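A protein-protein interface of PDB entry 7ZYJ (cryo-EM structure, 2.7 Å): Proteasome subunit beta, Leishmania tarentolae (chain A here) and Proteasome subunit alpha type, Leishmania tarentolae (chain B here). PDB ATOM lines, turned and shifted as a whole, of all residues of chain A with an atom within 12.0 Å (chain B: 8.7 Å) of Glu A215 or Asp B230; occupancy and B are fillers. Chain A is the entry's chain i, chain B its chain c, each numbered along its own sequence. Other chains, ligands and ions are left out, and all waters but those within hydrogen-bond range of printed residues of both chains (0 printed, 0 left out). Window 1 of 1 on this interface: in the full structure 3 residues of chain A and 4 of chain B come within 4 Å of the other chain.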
ATOM      1  N   PRO A 210       7.553  -8.639 -38.967  1.00  0.00           N
ATOM      2  CA  PRO A 210       7.564  -7.171 -38.905  1.00  0.00           C
ATOM      3  C   PRO A 210       7.533  -6.666 -37.470  1.00  0.00           C
ATOM      4  O   PRO A 210       6.924  -7.273 -36.587  1.00  0.00           O
ATOM      5  CB  PRO A 210       6.296  -6.774 -39.670  1.00  0.00           C
ATOM      6  CG  PRO A 210       5.412  -7.971 -39.588  1.00  0.00           C
ATOM      7  CD  PRO A 210       6.320  -9.163 -39.578  1.00  0.00           C
ATOM      8  N   VAL A 211       8.200  -5.535 -37.249  1.00  0.00           N
ATOM      9  CA  VAL A 211       8.347  -4.933 -35.930  1.00  0.00           C
ATOM     10  C   VAL A 211       7.783  -3.520 -35.980  1.00  0.00           C
ATOM     11  O   VAL A 211       8.034  -2.777 -36.936  1.00  0.00           O
ATOM     12  CB  VAL A 211       9.822  -4.927 -35.476  1.00  0.00           C
ATOM     13  CG1 VAL A 211      10.003  -4.087 -34.224  1.00  0.00           C
ATOM     14  CG2 VAL A 211      10.309  -6.350 -35.245  1.00  0.00           C
ATOM     15  N   LEU A 212       7.020  -3.151 -34.951  1.00  0.00           N
ATOM     16  CA  LEU A 212       6.296  -1.885 -34.946  1.00  0.00           C
ATOM     17  C   LEU A 212       7.101  -0.780 -34.259  1.00  0.00           C
ATOM     18  O   LEU A 212       7.291   0.296 -34.834  1.00  0.00           O
ATOM     19  CB  LEU A 212       4.922  -2.102 -34.295  1.00  0.00           C
ATOM     20  CG  LEU A 212       3.752  -1.121 -34.426  1.00  0.00           C
ATOM     21  CD1 LEU A 212       2.442  -1.886 -34.325  1.00  0.00           C
ATOM     22  CD2 LEU A 212       3.776  -0.077 -33.353  1.00  0.00           C
ATOM     23  N   LYS A 213       7.591  -1.030 -33.042  1.00  0.00           N
ATOM     24  CA  LYS A 213       8.646  -0.225 -32.435  1.00  0.00           C
ATOM     25  C   LYS A 213       9.736  -1.130 -31.880  1.00  0.00           C
ATOM     26  O   LYS A 213       9.502  -2.301 -31.571  1.00  0.00           O
ATOM     27  CB  LYS A 213       8.162   0.699 -31.299  1.00  0.00           C
ATOM     28  CG  LYS A 213       7.592   2.049 -31.720  1.00  0.00           C
ATOM     29  CD  LYS A 213       6.225   1.957 -32.332  1.00  0.00           C
ATOM     30  CE  LYS A 213       5.663   3.333 -32.643  1.00  0.00           C
ATOM     31  NZ  LYS A 213       4.362   3.251 -33.359  1.00  0.00           N
ATOM     32  N   GLU A 214      10.933  -0.560 -31.752  1.00  0.00           N
ATOM     33  CA  GLU A 214      12.086  -1.239 -31.185  1.00  0.00           C
ATOM     34  C   GLU A 214      12.803  -0.300 -30.225  1.00  0.00           C
ATOM     35  O   GLU A 214      12.926   0.900 -30.484  1.00  0.00           O
ATOM     36  CB  GLU A 214      13.057  -1.704 -32.279  1.00  0.00           C
ATOM     37  CG  GLU A 214      14.229  -2.522 -31.769  1.00  0.00           C
ATOM     38  CD  GLU A 214      14.740  -3.512 -32.794  1.00  0.00           C
ATOM     39  OE1 GLU A 214      13.922  -4.019 -33.591  1.00  0.00           O
ATOM     40  OE2 GLU A 214      15.958  -3.788 -32.801  1.00  0.00           O
ATOM     41  N   GLU A 215      13.274  -0.858 -29.111  1.00  0.00           N
ATOM     42  CA  GLU A 215      14.039  -0.102 -28.120  1.00  0.00           C
ATOM     43  C   GLU A 215      15.181  -0.980 -27.629  1.00  0.00           C
ATOM     44  O   GLU A 215      14.948  -2.095 -27.153  1.00  0.00           O
ATOM     45  CB  GLU A 215      13.158   0.349 -26.953  1.00  0.00           C
ATOM     46  CG  GLU A 215      12.003   1.255 -27.350  1.00  0.00           C
ATOM     47  CD  GLU A 215      11.653   2.262 -26.270  1.00  0.00           C
ATOM     48  OE1 GLU A 215      11.835   1.944 -25.076  1.00  0.00           O
ATOM     49  OE2 GLU A 215      11.195   3.371 -26.618  1.00  0.00           O
ATOM     50  N   ILE A 216      16.408  -0.479 -27.743  1.00  0.00           N
ATOM     51  CA  ILE A 216      17.603  -1.197 -27.313  1.00  0.00           C
ATOM     52  C   ILE A 216      18.186  -0.485 -26.102  1.00  0.00           C
ATOM     53  O   ILE A 216      18.364   0.740 -26.119  1.00  0.00           O
ATOM     54  CB  ILE A 216      18.636  -1.289 -28.449  1.00  0.00           C
ATOM     55  CG1 ILE A 216      18.013  -1.940 -29.684  1.00  0.00           C
ATOM     56  CG2 ILE A 216      19.857  -2.074 -27.995  1.00  0.00           C
ATOM     57  CD1 ILE A 216      18.842  -1.788 -30.939  1.00  0.00           C
ATOM     58  N   ARG A 217      18.486  -1.246 -25.051  1.00  0.00           N
ATOM     59  CA  ARG A 217      19.039  -0.701 -23.815  1.00  0.00           C
ATOM     60  C   ARG A 217      20.346  -1.420 -23.505  1.00  0.00           C
ATOM     61  O   ARG A 217      20.337  -2.598 -23.132  1.00  0.00           O
ATOM     62  CB  ARG A 217      18.051  -0.844 -22.657  1.00  0.00           C
ATOM     63  CG  ARG A 217      16.899   0.146 -22.699  1.00  0.00           C
ATOM     64  CD  ARG A 217      17.396   1.560 -22.954  1.00  0.00           C
ATOM     65  NE  ARG A 217      16.298   2.491 -23.187  1.00  0.00           N
ATOM     66  CZ  ARG A 217      15.858   3.367 -22.294  1.00  0.00           C
ATOM     67  NH1 ARG A 217      16.402   3.462 -21.092  1.00  0.00           N
ATOM     68  NH2 ARG A 217      14.845   4.167 -22.615  1.00  0.00           N
ATOM     69  N   GLN A 218      21.461  -0.713 -23.658  1.00  0.00           N
ATOM     70  CA  GLN A 218      22.767  -1.270 -23.341  1.00  0.00           C
ATOM     71  C   GLN A 218      22.979  -1.317 -21.833  1.00  0.00           C
ATOM     72  O   GLN A 218      22.524  -0.441 -21.091  1.00  0.00           O
ATOM     73  CB  GLN A 218      23.876  -0.446 -23.995  1.00  0.00           C
ATOM     74  CG  GLN A 218      23.753  -0.314 -25.503  1.00  0.00           C
ATOM     75  CD  GLN A 218      23.917  -1.639 -26.220  1.00  0.00           C
ATOM     76  OE1 GLN A 218      24.708  -2.487 -25.808  1.00  0.00           O
ATOM     77  NE2 GLN A 218      23.171  -1.822 -27.302  1.00  0.00           N
ATOM     78  N   LEU A 219      23.679  -2.352 -21.384  1.00  0.00           N
ATOM     79  CA  LEU A 219      23.990  -2.506 -19.967  1.00  0.00           C
ATOM     80  C   LEU A 219      25.496  -2.561 -19.740  1.00  0.00           C
ATOM     81  O   LEU A 219      26.125  -1.547 -19.433  1.00  0.00           O
ATOM     82  CB  LEU A 219      23.328  -3.765 -19.404  1.00  0.00           C
ATOM     83  CG  LEU A 219      21.868  -4.007 -19.790  1.00  0.00           C
ATOM     84  CD1 LEU A 219      21.381  -5.309 -19.192  1.00  0.00           C
ATOM     85  CD2 LEU A 219      20.990  -2.850 -19.340  1.00  0.00           C
ATOM     86  N   ALA B 226      16.753   9.459 -16.226  1.00  0.00           N
ATOM     87  CA  ALA B 226      16.235   8.107 -16.079  1.00  0.00           C
ATOM     88  C   ALA B 226      16.981   7.141 -16.995  1.00  0.00           C
ATOM     89  O   ALA B 226      17.398   7.493 -18.102  1.00  0.00           O
ATOM     90  CB  ALA B 226      14.739   8.078 -16.383  1.00  0.00           C
ATOM     91  N   SER B 227      17.144   5.908 -16.520  1.00  0.00           N
ATOM     92  CA  SER B 227      17.962   4.907 -17.194  1.00  0.00           C
ATOM     93  C   SER B 227      17.165   3.720 -17.714  1.00  0.00           C
ATOM     94  O   SER B 227      17.481   3.187 -18.781  1.00  0.00           O
ATOM     95  CB  SER B 227      19.062   4.412 -16.243  1.00  0.00           C
ATOM     96  OG  SER B 227      19.885   3.445 -16.872  1.00  0.00           O
ATOM     97  N   ASN B 228      16.132   3.291 -16.993  1.00  0.00           N
ATOM     98  CA  ASN B 228      15.421   2.050 -17.287  1.00  0.00           C
ATOM     99  C   ASN B 228      13.980   2.314 -17.722  1.00  0.00           C
ATOM    100  O   ASN B 228      13.045   1.648 -17.274  1.00  0.00           O
ATOM    101  CB  ASN B 228      15.457   1.113 -16.081  1.00  0.00           C
ATOM    102  CG  ASN B 228      15.070  -0.313 -16.431  1.00  0.00           C
ATOM    103  OD1 ASN B 228      14.767  -0.623 -17.583  1.00  0.00           O
ATOM    104  ND2 ASN B 228      15.082  -1.191 -15.434  1.00  0.00           N
ATOM    105  N   ILE B 229      13.785   3.298 -18.593  1.00  0.00           N
ATOM    106  CA  ILE B 229      12.460   3.602 -19.125  1.00  0.00           C
ATOM    107  C   ILE B 229      12.155   2.614 -20.246  1.00  0.00           C
ATOM    108  O   ILE B 229      12.856   2.573 -21.259  1.00  0.00           O
ATOM    109  CB  ILE B 229      12.369   5.049 -19.622  1.00  0.00           C
ATOM    110  CG1 ILE B 229      12.750   6.020 -18.504  1.00  0.00           C
ATOM    111  CG2 ILE B 229      10.974   5.345 -20.151  1.00  0.00           C
ATOM    112  CD1 ILE B 229      12.019   5.770 -17.201  1.00  0.00           C
ATOM    113  N   ASP B 230      11.106   1.815 -20.064  1.00  0.00           N
ATOM    114  CA  ASP B 230      10.640   0.867 -21.075  1.00  0.00           C
ATOM    115  C   ASP B 230       9.153   1.128 -21.301  1.00  0.00           C
ATOM    116  O   ASP B 230       8.304   0.580 -20.591  1.00  0.00           O
ATOM    117  CB  ASP B 230      10.902  -0.573 -20.643  1.00  0.00           C
ATOM    118  CG  ASP B 230      10.828  -1.550 -21.801  1.00  0.00           C
ATOM    119  OD1 ASP B 230      10.601  -1.102 -22.945  1.00  0.00           O
ATOM    120  OD2 ASP B 230      11.003  -2.764 -21.569  1.00  0.00           O
ATOM    121  N   GLN B 231       8.844   1.965 -22.294  1.00  0.00           N
ATOM    122  CA  GLN B 231       7.460   2.362 -22.532  1.00  0.00           C
ATOM    123  C   GLN B 231       6.639   1.240 -23.154  1.00  0.00           C
ATOM    124  O   GLN B 231       5.420   1.186 -22.957  1.00  0.00           O
ATOM    125  CB  GLN B 231       7.421   3.603 -23.425  1.00  0.00           C
ATOM    126  CG  GLN B 231       6.075   4.308 -23.465  1.00  0.00           C
ATOM    127  CD  GLN B 231       5.762   5.049 -22.182  1.00  0.00           C
ATOM    128  OE1 GLN B 231       6.094   6.226 -22.036  1.00  0.00           O
ATOM    129  NE2 GLN B 231       5.117   4.365 -21.245  1.00  0.00           N
ATOM    130  N   LEU B 232       7.280   0.339 -23.901  1.00  0.00           N
ATOM    131  CA  LEU B 232       6.545  -0.713 -24.597  1.00  0.00           C
ATOM    132  C   LEU B 232       5.895  -1.710 -23.646  1.00  0.00           C
ATOM    133  O   LEU B 232       4.917  -2.359 -24.029  1.00  0.00           O
ATOM    134  CB  LEU B 232       7.468  -1.454 -25.564  1.00  0.00           C
ATOM    135  CG  LEU B 232       7.626  -0.865 -26.967  1.00  0.00           C
ATOM    136  CD1 LEU B 232       8.504   0.371 -26.938  1.00  0.00           C
ATOM    137  CD2 LEU B 232       8.194  -1.903 -27.922  1.00  0.00           C
ATOM    138  N   LEU B 233       6.411  -1.853 -22.427  1.00  0.00           N
ATOM    139  CA  LEU B 233       5.854  -2.809 -21.479  1.00  0.00           C
ATOM    140  C   LEU B 233       4.609  -2.300 -20.766  1.00  0.00           C
ATOM    141  O   LEU B 233       3.889  -3.104 -20.166  1.00  0.00           O
ATOM    142  CB  LEU B 233       6.901  -3.199 -20.435  1.00  0.00           C
ATOM    143  CG  LEU B 233       8.065  -4.066 -20.913  1.00  0.00           C
ATOM    144  CD1 LEU B 233       8.693  -4.762 -19.724  1.00  0.00           C
ATOM    145  CD2 LEU B 233       7.607  -5.080 -21.946  1.00  0.00           C
ATOM    146  N   ASP B 234       4.344  -0.998 -20.800  1.00  0.00           N
ATOM    147  CA  ASP B 234       3.088  -0.447 -20.291  1.00  0.00           C
ATOM    148  C   ASP B 234       2.889   0.911 -20.942  1.00  0.00           C
ATOM    149  O   ASP B 234       3.306   1.947 -20.409  1.00  0.00           O
ATOM    150  CB  ASP B 234       3.097  -0.340 -18.766  1.00  0.00           C
ATOM    151  CG  ASP B 234       1.755   0.082 -18.206  1.00  0.00           C
ATOM    152  OD1 ASP B 234       0.832  -0.756 -18.189  1.00  0.00           O
ATOM    153  OD2 ASP B 234       1.606   1.245 -17.792  1.00  0.00           O
ATOM    154  N   PRO B 235       2.257   0.943 -22.118  1.00  0.00           N
ATOM    155  CA  PRO B 235       2.255   2.166 -22.936  1.00  0.00           C
ATOM    156  C   PRO B 235       1.564   3.359 -22.293  1.00  0.00           C
ATOM    157  O   PRO B 235       1.771   4.498 -22.722  1.00  0.00           O
ATOM    158  CB  PRO B 235       1.521   1.728 -24.211  1.00  0.00           C
ATOM    159  CG  PRO B 235       1.625   0.231 -24.226  1.00  0.00           C
ATOM    160  CD  PRO B 235       1.592  -0.181 -22.795  1.00  0.00           C
ATOM    161  N   PHE B 236       0.748   3.123 -21.267  1.00  0.00           N
ATOM    162  CA  PHE B 236      -0.035   4.185 -20.652  1.00  0.00           C
ATOM    163  C   PHE B 236       0.613   4.788 -19.413  1.00  0.00           C
ATOM    164  O   PHE B 236       0.034   5.704 -18.816  1.00  0.00           O
ATOM    165  CB  PHE B 236      -1.433   3.665 -20.292  1.00  0.00           C
ATOM    166  CG  PHE B 236      -2.295   3.363 -21.486  1.00  0.00           C
ATOM    167  CD1 PHE B 236      -3.073   4.352 -22.066  1.00  0.00           C
ATOM    168  CD2 PHE B 236      -2.327   2.090 -22.027  1.00  0.00           C
ATOM    169  CE1 PHE B 236      -3.865   4.074 -23.164  1.00  0.00           C
ATOM    170  CE2 PHE B 236      -3.117   1.805 -23.126  1.00  0.00           C
ATOM    171  CZ  PHE B 236      -3.887   2.799 -23.694  1.00  0.00           C
ATOM    172  N   LYS B 237       1.791   4.319 -19.010  1.00  0.00           N
ATOM    173  CA  LYS B 237       2.447   4.820 -17.808  1.00  0.00           C
ATOM    174  C   LYS B 237       3.402   5.945 -18.187  1.00  0.00           C
ATOM    175  O   LYS B 237       4.277   5.763 -19.041  1.00  0.00           O
ATOM    176  CB  LYS B 237       3.196   3.702 -17.085  1.00  0.00           C
ATOM    177  CG  LYS B 237       3.482   3.978 -15.616  1.00  0.00           C
ATOM    178  CD  LYS B 237       4.848   4.601 -15.409  1.00  0.00           C
ATOM    179  CE  LYS B 237       5.136   4.811 -13.933  1.00  0.00           C
ATOM    180  NZ  LYS B 237       6.446   5.482 -13.708  1.00  0.00           N
ATOM    181  N   HIS B 239       6.545   8.120 -17.671  1.00  0.00           N
ATOM    182  CA  HIS B 239       7.846   7.967 -17.033  1.00  0.00           C
ATOM    183  C   HIS B 239       8.555   9.307 -16.970  1.00  0.00           C
ATOM    184  O   HIS B 239       8.796   9.920 -18.020  1.00  0.00           O
ATOM    185  CB  HIS B 239       8.706   6.967 -17.799  1.00  0.00           C
ATOM    186  CG  HIS B 239       8.030   5.657 -18.056  1.00  0.00           C
ATOM    187  ND1 HIS B 239       7.965   4.655 -17.113  1.00  0.00           N
ATOM    188  CD2 HIS B 239       7.391   5.185 -19.152  1.00  0.00           C
ATOM    189  CE1 HIS B 239       7.316   3.621 -17.617  1.00  0.00           C
ATOM    190  NE2 HIS B 239       6.955   3.917 -18.853  1.00  0.00           N
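O of Ser B227 is in hydrogen-bond range of NH1 of Arg A217 (2.6 Å). NH2 of Arg A217 is in hydrogen-bond range of O of Ile B229, at 2.9 Å.
Of chain A, only Glu A215 (3.9 Å) comes within 4 Å of Asp B230. Leu B232 touches two residues of chain A. No residue of chain A comes within 4 Å of Leu B233. No residue of chain A comes within 4 Å of Pro B235. Of the printed residues of chain B, Lys A213 touches Leu B232. Printed residues of chain A within 4 Å of Ile B229: Arg A217 (2.9 Å). Of the printed residues of chain B, Arg A217 touches Ser B227 and Ile B229. Of the printed residues of chain A, Ser B227 touches Arg A217. Gln A218 touches none of the printed residues of chain B. The nearest printed residue of chain B that does not touch Glu A215 is Ile B229 (4.001 Å).
Of the 13 printed residues of chain B, 4 touch a printed residue of chain A. Printed residues of chain B that touch a printed residue of chain A: Ser B227, Ile B229, Asp B230 and Leu B232. Among the printed residues, no Asp or Glu carboxylate lies within 4 Å of a Lys or Arg side-chain nitrogen of the other chain.
Among the printed residues, merely in contact across the chains: Glu A215 with Leu B232 (3.6 Å), Lys A213 with Leu B232 (3.9 Å) and Glu A215 with Asp B230 (3.9 Å).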
